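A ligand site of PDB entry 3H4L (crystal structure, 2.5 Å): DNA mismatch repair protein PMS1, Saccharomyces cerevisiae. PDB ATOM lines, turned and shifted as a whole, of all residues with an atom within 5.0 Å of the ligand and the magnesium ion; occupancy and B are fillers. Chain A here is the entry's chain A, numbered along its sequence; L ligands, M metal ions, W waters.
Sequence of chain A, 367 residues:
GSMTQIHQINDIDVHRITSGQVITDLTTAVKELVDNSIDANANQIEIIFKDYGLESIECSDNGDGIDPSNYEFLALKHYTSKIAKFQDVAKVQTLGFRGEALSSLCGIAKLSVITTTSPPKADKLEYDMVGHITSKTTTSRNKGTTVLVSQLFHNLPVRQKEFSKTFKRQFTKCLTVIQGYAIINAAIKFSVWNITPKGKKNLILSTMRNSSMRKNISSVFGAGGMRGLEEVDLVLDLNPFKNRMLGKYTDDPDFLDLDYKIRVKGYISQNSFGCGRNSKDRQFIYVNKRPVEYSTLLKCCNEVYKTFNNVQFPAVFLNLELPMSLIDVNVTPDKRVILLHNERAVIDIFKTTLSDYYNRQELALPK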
ATOM      1  N   GLU A  32      -5.531  -5.521  21.173  1.00  0.00           N
ATOM      2  CA  GLU A  32      -4.155  -5.117  21.034  1.00  0.00           C
ATOM      3  C   GLU A  32      -4.011  -3.625  21.336  1.00  0.00           C
ATOM      4  O   GLU A  32      -3.159  -3.226  22.134  1.00  0.00           O
ATOM      5  CB  GLU A  32      -3.636  -5.431  19.639  1.00  0.00           C
ATOM      6  CG  GLU A  32      -3.555  -6.928  19.347  1.00  0.00           C
ATOM      7  CD  GLU A  32      -2.963  -7.740  20.489  1.00  0.00           C
ATOM      8  OE1 GLU A  32      -2.189  -7.178  21.297  1.00  0.00           O
ATOM      9  OE2 GLU A  32      -3.248  -8.954  20.583  1.00  0.00           O
ATOM     10  N   ASP A  35      -5.002  -2.600  25.145  1.00  0.00           N
ATOM     11  CA  ASP A  35      -3.975  -3.068  26.069  1.00  0.00           C
ATOM     12  C   ASP A  35      -2.752  -2.155  26.015  1.00  0.00           C
ATOM     13  O   ASP A  35      -2.156  -1.834  27.047  1.00  0.00           O
ATOM     14  CB  ASP A  35      -3.520  -4.485  25.729  1.00  0.00           C
ATOM     15  CG  ASP A  35      -4.271  -5.545  26.495  1.00  0.00           C
ATOM     16  OD1 ASP A  35      -5.045  -5.206  27.422  1.00  0.00           O
ATOM     17  OD2 ASP A  35      -4.076  -6.752  26.196  1.00  0.00           O
ATOM     18  N   ASN A  36      -2.382  -1.744  24.801  1.00  0.00           N
ATOM     19  CA  ASN A  36      -1.242  -0.863  24.670  1.00  0.00           C
ATOM     20  C   ASN A  36      -1.512   0.472  25.372  1.00  0.00           C
ATOM     21  O   ASN A  36      -0.696   0.952  26.138  1.00  0.00           O
ATOM     22  CB  ASN A  36      -0.884  -0.670  23.202  1.00  0.00           C
ATOM     23  CG  ASN A  36      -0.264  -1.933  22.582  1.00  0.00           C
ATOM     24  OD1 ASN A  36       0.195  -2.830  23.310  1.00  0.00           O
ATOM     25  ND2 ASN A  36      -0.241  -2.015  21.258  1.00  0.00           N
ATOM     26  N   SER A  37      -2.683   1.069  25.144  1.00  0.00           N
ATOM     27  CA  SER A  37      -2.987   2.321  25.813  1.00  0.00           C
ATOM     28  C   SER A  37      -2.949   2.131  27.343  1.00  0.00           C
ATOM     29  O   SER A  37      -2.327   2.920  28.047  1.00  0.00           O
ATOM     30  CB  SER A  37      -4.349   2.830  25.378  1.00  0.00           C
ATOM     31  OG  SER A  37      -4.355   3.109  23.997  1.00  0.00           O
ATOM     32  N   ASP A  39      -1.370  -0.062  28.981  1.00  0.00           N
ATOM     33  CA  ASP A  39       0.009  -0.339  29.343  1.00  0.00           C
ATOM     34  C   ASP A  39       0.767   0.984  29.410  1.00  0.00           C
ATOM     35  O   ASP A  39       1.761   1.109  30.124  1.00  0.00           O
ATOM     36  CB  ASP A  39       0.677  -1.232  28.299  1.00  0.00           C
ATOM     37  CG  ASP A  39       0.260  -2.704  28.395  1.00  0.00           C
ATOM     38  OD1 ASP A  39      -0.414  -3.090  29.388  1.00  0.00           O
ATOM     39  OD2 ASP A  39       0.624  -3.462  27.468  1.00  0.00           O
ATOM     40  N   ALA A  40       0.291   1.971  28.661  1.00  0.00           N
ATOM     41  CA  ALA A  40       0.944   3.266  28.593  1.00  0.00           C
ATOM     42  C   ALA A  40       0.521   4.210  29.701  1.00  0.00           C
ATOM     43  O   ALA A  40       0.847   5.407  29.667  1.00  0.00           O
ATOM     44  CB  ALA A  40       0.680   3.885  27.231  1.00  0.00           C
ATOM     45  N   ASP A  61      -5.278   7.691  23.317  1.00  0.00           N
ATOM     46  CA  ASP A  61      -5.061   7.669  24.754  1.00  0.00           C
ATOM     47  C   ASP A  61      -4.259   8.899  25.206  1.00  0.00           C
ATOM     48  O   ASP A  61      -3.683   9.618  24.394  1.00  0.00           O
ATOM     49  CB  ASP A  61      -4.290   6.400  25.134  1.00  0.00           C
ATOM     50  CG  ASP A  61      -2.849   6.407  24.630  1.00  0.00           C
ATOM     51  OD1 ASP A  61      -2.122   7.378  24.914  1.00  0.00           O
ATOM     52  OD2 ASP A  61      -2.438   5.435  23.947  1.00  0.00           O
ATOM     53  N   ASP A  64       1.651   7.839  28.294  1.00  0.00           N
ATOM     54  CA  ASP A  64       2.894   8.576  28.380  1.00  0.00           C
ATOM     55  C   ASP A  64       3.649   8.680  27.050  1.00  0.00           C
ATOM     56  O   ASP A  64       4.822   9.043  27.019  1.00  0.00           O
ATOM     57  CB  ASP A  64       3.795   8.007  29.489  1.00  0.00           C
ATOM     58  CG  ASP A  64       4.102   6.531  29.320  1.00  0.00           C
ATOM     59  OD1 ASP A  64       4.497   6.118  28.199  1.00  0.00           O
ATOM     60  OD2 ASP A  64       3.970   5.787  30.330  1.00  0.00           O
ATOM     61  N   GLY A  65       2.941   8.383  25.953  1.00  0.00           N
ATOM     62  CA  GLY A  65       3.518   8.477  24.621  1.00  0.00           C
ATOM     63  C   GLY A  65       4.578   7.453  24.263  1.00  0.00           C
ATOM     64  O   GLY A  65       4.946   6.598  25.063  1.00  0.00           O
ATOM     65  N   ILE A  66       5.069   7.551  23.026  1.00  0.00           N
ATOM     66  CA  ILE A  66       6.117   6.669  22.513  1.00  0.00           C
ATOM     67  C   ILE A  66       7.405   7.465  22.408  1.00  0.00           C
ATOM     68  O   ILE A  66       7.477   8.435  21.646  1.00  0.00           O
ATOM     69  CB  ILE A  66       5.799   6.136  21.095  1.00  0.00           C
ATOM     70  CG1 ILE A  66       4.416   5.494  21.059  1.00  0.00           C
ATOM     71  CG2 ILE A  66       6.859   5.142  20.665  1.00  0.00           C
ATOM     72  CD1 ILE A  66       4.028   4.927  19.695  1.00  0.00           C
ATOM     73  N   ASN A  70      12.030   4.681  20.239  1.00  0.00           N
ATOM     74  CA  ASN A  70      11.343   3.442  19.894  1.00  0.00           C
ATOM     75  C   ASN A  70      10.694   3.454  18.521  1.00  0.00           C
ATOM     76  O   ASN A  70      10.301   2.403  18.029  1.00  0.00           O
ATOM     77  CB  ASN A  70      10.286   3.102  20.955  1.00  0.00           C
ATOM     78  CG  ASN A  70      10.894   2.649  22.269  1.00  0.00           C
ATOM     79  OD1 ASN A  70      11.858   1.885  22.292  1.00  0.00           O
ATOM     80  ND2 ASN A  70      10.323   3.111  23.371  1.00  0.00           N
ATOM     81  N   LEU A  74       9.260   0.249  16.547  1.00  0.00           N
ATOM     82  CA  LEU A  74       7.896   0.283  17.050  1.00  0.00           C
ATOM     83  C   LEU A  74       7.014  -0.844  16.543  1.00  0.00           C
ATOM     84  O   LEU A  74       6.274  -1.458  17.314  1.00  0.00           O
ATOM     85  CB  LEU A  74       7.218   1.605  16.692  1.00  0.00           C
ATOM     86  CG  LEU A  74       5.765   1.664  17.152  1.00  0.00           C
ATOM     87  CD1 LEU A  74       5.722   1.553  18.676  1.00  0.00           C
ATOM     88  CD2 LEU A  74       5.105   2.956  16.671  1.00  0.00           C
ATOM     89  N   LEU A  95       1.708 -12.551  29.413  1.00  0.00           N
ATOM     90  CA  LEU A  95       2.781 -12.884  28.498  1.00  0.00           C
ATOM     91  C   LEU A  95       2.745 -11.835  27.411  1.00  0.00           C
ATOM     92  O   LEU A  95       1.662 -11.385  27.017  1.00  0.00           O
ATOM     93  CB  LEU A  95       2.580 -14.260  27.885  1.00  0.00           C
ATOM     94  CG  LEU A  95       3.894 -14.949  27.529  1.00  0.00           C
ATOM     95  CD1 LEU A  95       4.682 -15.177  28.792  1.00  0.00           C
ATOM     96  CD2 LEU A  95       3.642 -16.265  26.802  1.00  0.00           C
ATOM     97  N   GLY A  96       3.912 -11.443  26.943  1.00  0.00           N
ATOM     98  CA  GLY A  96       3.971 -10.442  25.898  1.00  0.00           C
ATOM     99  C   GLY A  96       4.960 -10.779  24.812  1.00  0.00           C
ATOM    100  O   GLY A  96       5.945 -11.485  25.040  1.00  0.00           O
ATOM    101  N   PHE A  97       4.676 -10.297  23.610  1.00  0.00           N
ATOM    102  CA  PHE A  97       5.557 -10.506  22.473  1.00  0.00           C
ATOM    103  C   PHE A  97       5.710  -9.144  21.821  1.00  0.00           C
ATOM    104  O   PHE A  97       5.026  -8.805  20.848  1.00  0.00           O
ATOM    105  CB  PHE A  97       4.966 -11.530  21.514  1.00  0.00           C
ATOM    106  CG  PHE A  97       4.835 -12.904  22.109  1.00  0.00           C
ATOM    107  CD1 PHE A  97       3.663 -13.290  22.753  1.00  0.00           C
ATOM    108  CD2 PHE A  97       5.906 -13.804  22.059  1.00  0.00           C
ATOM    109  CE1 PHE A  97       3.564 -14.557  23.344  1.00  0.00           C
ATOM    110  CE2 PHE A  97       5.807 -15.070  22.650  1.00  0.00           C
ATOM    111  CZ  PHE A  97       4.631 -15.447  23.284  1.00  0.00           C
ATOM    112  N   ARG A  98       6.628  -8.368  22.391  1.00  0.00           N
ATOM    113  CA  ARG A  98       6.905  -7.021  21.946  1.00  0.00           C
ATOM    114  C   ARG A  98       6.984  -6.851  20.443  1.00  0.00           C
ATOM    115  O   ARG A  98       7.763  -7.520  19.769  1.00  0.00           O
ATOM    116  CB  ARG A  98       8.208  -6.530  22.559  1.00  0.00           C
ATOM    117  CG  ARG A  98       8.451  -5.067  22.321  1.00  0.00           C
ATOM    118  CD  ARG A  98       9.902  -4.724  22.526  1.00  0.00           C
ATOM    119  NE  ARG A  98      10.092  -3.308  22.772  1.00  0.00           N
ATOM    120  CZ  ARG A  98      11.282  -2.757  22.995  1.00  0.00           C
ATOM    121  NH1 ARG A  98      12.363  -3.518  22.998  1.00  0.00           N
ATOM    122  NH2 ARG A  98      11.373  -1.450  23.249  1.00  0.00           N
ATOM    123  N   GLY A  99       6.171  -5.932  19.928  1.00  0.00           N
ATOM    124  CA  GLY A  99       6.153  -5.666  18.509  1.00  0.00           C
ATOM    125  C   GLY A  99       5.269  -6.592  17.699  1.00  0.00           C
ATOM    126  O   GLY A  99       4.839  -6.239  16.614  1.00  0.00           O
ATOM    127  N   GLU A 100       4.980  -7.773  18.231  1.00  0.00           N
ATOM    128  CA  GLU A 100       4.148  -8.715  17.497  1.00  0.00           C
ATOM    129  C   GLU A 100       2.820  -8.111  17.047  1.00  0.00           C
ATOM    130  O   GLU A 100       2.503  -8.102  15.853  1.00  0.00           O
ATOM    131  CB  GLU A 100       3.865  -9.951  18.353  1.00  0.00           C
ATOM    132  CG  GLU A 100       3.150 -11.062  17.599  1.00  0.00           C
ATOM    133  CD  GLU A 100       2.657 -12.164  18.508  1.00  0.00           C
ATOM    134  OE1 GLU A 100       1.752 -11.895  19.331  1.00  0.00           O
ATOM    135  OE2 GLU A 100       3.187 -13.291  18.404  1.00  0.00           O
ATOM    136  N   ALA A 101       2.031  -7.604  17.993  1.00  0.00           N
ATOM    137  CA  ALA A 101       0.753  -7.001  17.653  1.00  0.00           C
ATOM    138  C   ALA A 101       0.876  -5.918  16.588  1.00  0.00           C
ATOM    139  O   ALA A 101       0.226  -5.998  15.558  1.00  0.00           O
ATOM    140  CB  ALA A 101       0.103  -6.436  18.908  1.00  0.00           C
ATOM    141  N   LEU A 102       1.713  -4.915  16.830  1.00  0.00           N
ATOM    142  CA  LEU A 102       1.859  -3.830  15.867  1.00  0.00           C
ATOM    143  C   LEU A 102       2.415  -4.207  14.501  1.00  0.00           C
ATOM    144  O   LEU A 102       1.981  -3.660  13.485  1.00  0.00           O
ATOM    145  CB  LEU A 102       2.706  -2.688  16.451  1.00  0.00           C
ATOM    146  CG  LEU A 102       2.056  -1.806  17.509  1.00  0.00           C
ATOM    147  CD1 LEU A 102       2.925  -0.570  17.703  1.00  0.00           C
ATOM    148  CD2 LEU A 102       0.646  -1.392  17.085  1.00  0.00           C
ATOM    149  N   THR A 145      -0.909   9.085  22.807  1.00  0.00           N
ATOM    150  CA  THR A 145      -0.789   8.399  21.541  1.00  0.00           C
ATOM    151  C   THR A 145      -2.127   8.077  20.866  1.00  0.00           C
ATOM    152  O   THR A 145      -3.098   7.700  21.533  1.00  0.00           O
ATOM    153  CB  THR A 145      -0.038   7.073  21.719  1.00  0.00           C
ATOM    154  OG1 THR A 145       1.245   7.318  22.304  1.00  0.00           O
ATOM    155  CG2 THR A 145       0.121   6.363  20.386  1.00  0.00           C
ATOM    156  N   VAL A 147      -3.445   5.753  17.765  1.00  0.00           N
ATOM    157  CA  VAL A 147      -3.106   4.729  16.804  1.00  0.00           C
ATOM    158  C   VAL A 147      -4.275   4.557  15.835  1.00  0.00           C
ATOM    159  O   VAL A 147      -5.419   4.400  16.261  1.00  0.00           O
ATOM    160  CB  VAL A 147      -2.835   3.392  17.500  1.00  0.00           C
ATOM    161  CG1 VAL A 147      -2.299   2.378  16.494  1.00  0.00           C
ATOM    162  CG2 VAL A 147      -1.855   3.588  18.621  1.00  0.00           C
ATOM    163  N   LYS A 335      -1.455 -15.678  23.363  1.00  0.00           N
ATOM    164  CA  LYS A 335      -0.679 -15.050  24.419  1.00  0.00           C
ATOM    165  C   LYS A 335      -1.492 -14.613  25.638  1.00  0.00           C
ATOM    166  O   LYS A 335      -0.933 -14.452  26.726  1.00  0.00           O
ATOM    167  CB  LYS A 335       0.082 -13.837  23.868  1.00  0.00           C
ATOM    168  CG  LYS A 335      -0.813 -12.662  23.507  1.00  0.00           C
ATOM    169  CD  LYS A 335      -0.027 -11.496  22.934  1.00  0.00           C
ATOM    170  CE  LYS A 335      -0.932 -10.336  22.603  1.00  0.00           C
ATOM    171  NZ  LYS A 335      -0.186  -9.181  22.065  1.00  0.00           N
HETATM  172  P1  LIG L   1       2.103  -7.435  23.948  1.00  0.00           P
HETATM  173  O1  LIG L   1       1.385  -6.960  22.764  1.00  0.00           O
HETATM  174  O2  LIG L   1       1.469  -7.056  25.196  1.00  0.00           O
HETATM  175  O3  LIG L   1       2.391  -8.894  23.950  1.00  0.00           O
HETATM  176  P2  LIG L   1       3.821  -5.149  23.599  1.00  0.00           P
HETATM  177  O4  LIG L   1       5.218  -4.841  24.010  1.00  0.00           O
HETATM  178  O5  LIG L   1       2.810  -4.215  24.075  1.00  0.00           O
HETATM  179  N1  LIG L   1       3.541  -6.693  23.945  1.00  0.00           N
HETATM  180  P3  LIG L   1       2.952  -4.300  20.926  1.00  0.00           P
HETATM  181  O6  LIG L   1       1.546  -4.348  21.321  1.00  0.00           O
HETATM  182  O7  LIG L   1       3.322  -4.639  19.525  1.00  0.00           O
HETATM  183  O8  LIG L   1       3.813  -5.135  21.996  1.00  0.00           O
HETATM  184  O9  LIG L   1       3.502  -2.776  20.946  1.00  0.00           O
HETATM  185  C1  LIG L   1       4.718  -2.602  21.622  1.00  0.00           C
HETATM  186  C2  LIG L   1       5.524  -1.380  21.876  1.00  0.00           C
HETATM  187  O10 LIG L   1       4.969  -0.238  21.219  1.00  0.00           O
HETATM  188  C3  LIG L   1       5.247  -1.249  23.330  1.00  0.00           C
HETATM  189  O11 LIG L   1       6.110  -2.131  24.068  1.00  0.00           O
HETATM  190  C4  LIG L   1       5.354   0.257  23.561  1.00  0.00           C
HETATM  191  O12 LIG L   1       6.691   0.590  23.877  1.00  0.00           O
HETATM  192  C5  LIG L   1       4.840   0.794  22.198  1.00  0.00           C
HETATM  193  N2  LIG L   1       3.411   1.221  22.131  1.00  0.00           N
HETATM  194  C6  LIG L   1       2.316   0.724  21.433  1.00  0.00           C
HETATM  195  N3  LIG L   1       1.182   1.332  21.599  1.00  0.00           N
HETATM  196  C7  LIG L   1       1.525   2.353  22.470  1.00  0.00           C
HETATM  197  C8  LIG L   1       0.796   3.428  23.108  1.00  0.00           C
HETATM  198  N4  LIG L   1      -0.495   3.611  22.876  1.00  0.00           N
HETATM  199  N5  LIG L   1       1.446   4.309  23.975  1.00  0.00           N
HETATM  200  C9  LIG L   1       2.791   4.154  24.231  1.00  0.00           C
HETATM  201  N6  LIG L   1       3.562   3.167  23.677  1.00  0.00           N
HETATM  202  C10 LIG L   1       2.892   2.301  22.833  1.00  0.00           C
HETATM  203 MG    MG M   1       0.772  -4.953  23.255  1.00  0.00          MG
HETATM  204  O   HOH W   1       2.445  -2.191  25.877  1.00  0.00           O
HETATM  205  O   HOH W   2      -1.152  -4.932  22.428  1.00  0.00           O
HETATM  206  O   HOH W   3      -1.103   0.536  20.025  1.00  0.00           O
HETATM  207  O   HOH W   4       0.370  -8.978  26.399  1.00  0.00           O
HETATM  208  O   HOH W   5      -0.048  -4.760  25.317  1.00  0.00           O
HETATM  209  O   HOH W   6       0.423   6.847  25.122  1.00  0.00           O
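Water W2 bridges O of Glu 32 (2.7 Å) and ND2 of Asn 36 (3.3 Å). Water W5 bridges OD2 of Asp 39 (2.6 Å) and O2 of the ligand (2.8 Å). Water W4 lies within hydrogen-bond range of O2 of the ligand and O of Leu 95. Water W3 lies within hydrogen-bond range of N3 of the ligand and ND2 of Asn 36. Water W6 lies within hydrogen-bond range of the side-chain carboxylate (OD1) of Asp 61 (2.6 Å), a nitrogen (N5) of the ligand (3.0 Å), the side-chain hydroxyl (OG1) of Thr 145 (3.0 Å) and the backbone NH (N) of Gly 65 (3.1 Å).
One residue has an atom within 4 Å of the magnesium ion: Asn 36. The nearest printed residue that does not touch the magnesium ion is Glu 32 (4.2 Å).
The magnesium ion is bound by water W2 (2.1 Å), O1 of the ligand (2.2 Å), O6 of the ligand (2.2 Å), OD1 of Asn 36 (2.2 Å), water W5 (2.2 Å) and O5 of the ligand (2.3 Å).
Glu 32 touches the ligand. Ala 40 touches the ligand. O of Gly 65 touches C9 of the ligand, at 3.4 Å. Ile 66 touches the ligand (CG1 to N6, 3.6 Å). CD1 of Leu 74 touches O10 of the ligand, 3.2 Å away. CA of Gly 96 touches O3 of the ligand (2.9 Å). Arg 98 touches the ligand. Glu 100 touches the ligand (N to O7, 3.8 Å). Ala 101 touches the ligand (CB to O6, 3.5 Å). Of the 23 residues printed, 16 come within 4 Å of the ligand. The nearest printed residue that does not touch the ligand is Leu 95 (4.02 Å).
N of Phe 97 lies within hydrogen-bond range of O3 of the ligand. The side-chain amino group of Lys 335 lies within salt-bridge range of an oxygen (O3) of the ligand (3.2 Å). The side-chain carboxylate (OD2) of Asp 61 lies within hydrogen-bond range of a nitrogen (N4) of the ligand. N of Leu 102 lies within hydrogen-bond range of O7 of the ligand, at 3.2 Å. N of Gly 99 is in hydrogen-bond range of O7 of the ligand (3.2 Å). A nitrogen (N5) of the ligand lies within hydrogen-bond range of the side-chain hydroxyl (OG1) of Thr 145 (3.4 Å).
ND2 of Asn 36 lies close to O of Glu 32. The side-chain amino group of Lys 335 is in salt-bridge range of the side-chain carboxylate of Glu 32 (2.9 Å). The backbone NH of Asp 61 sits at hydrogen-bond distance from the backbone carbonyl oxygen of Thr 145 (2.8 Å). The side-chain carboxylate of Asp 61 sits at hydrogen-bond distance from the side-chain hydroxyl of Ser 37. O of Ala 40 lies within hydrogen-bond range of N of Asp 64 (2.9 Å).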
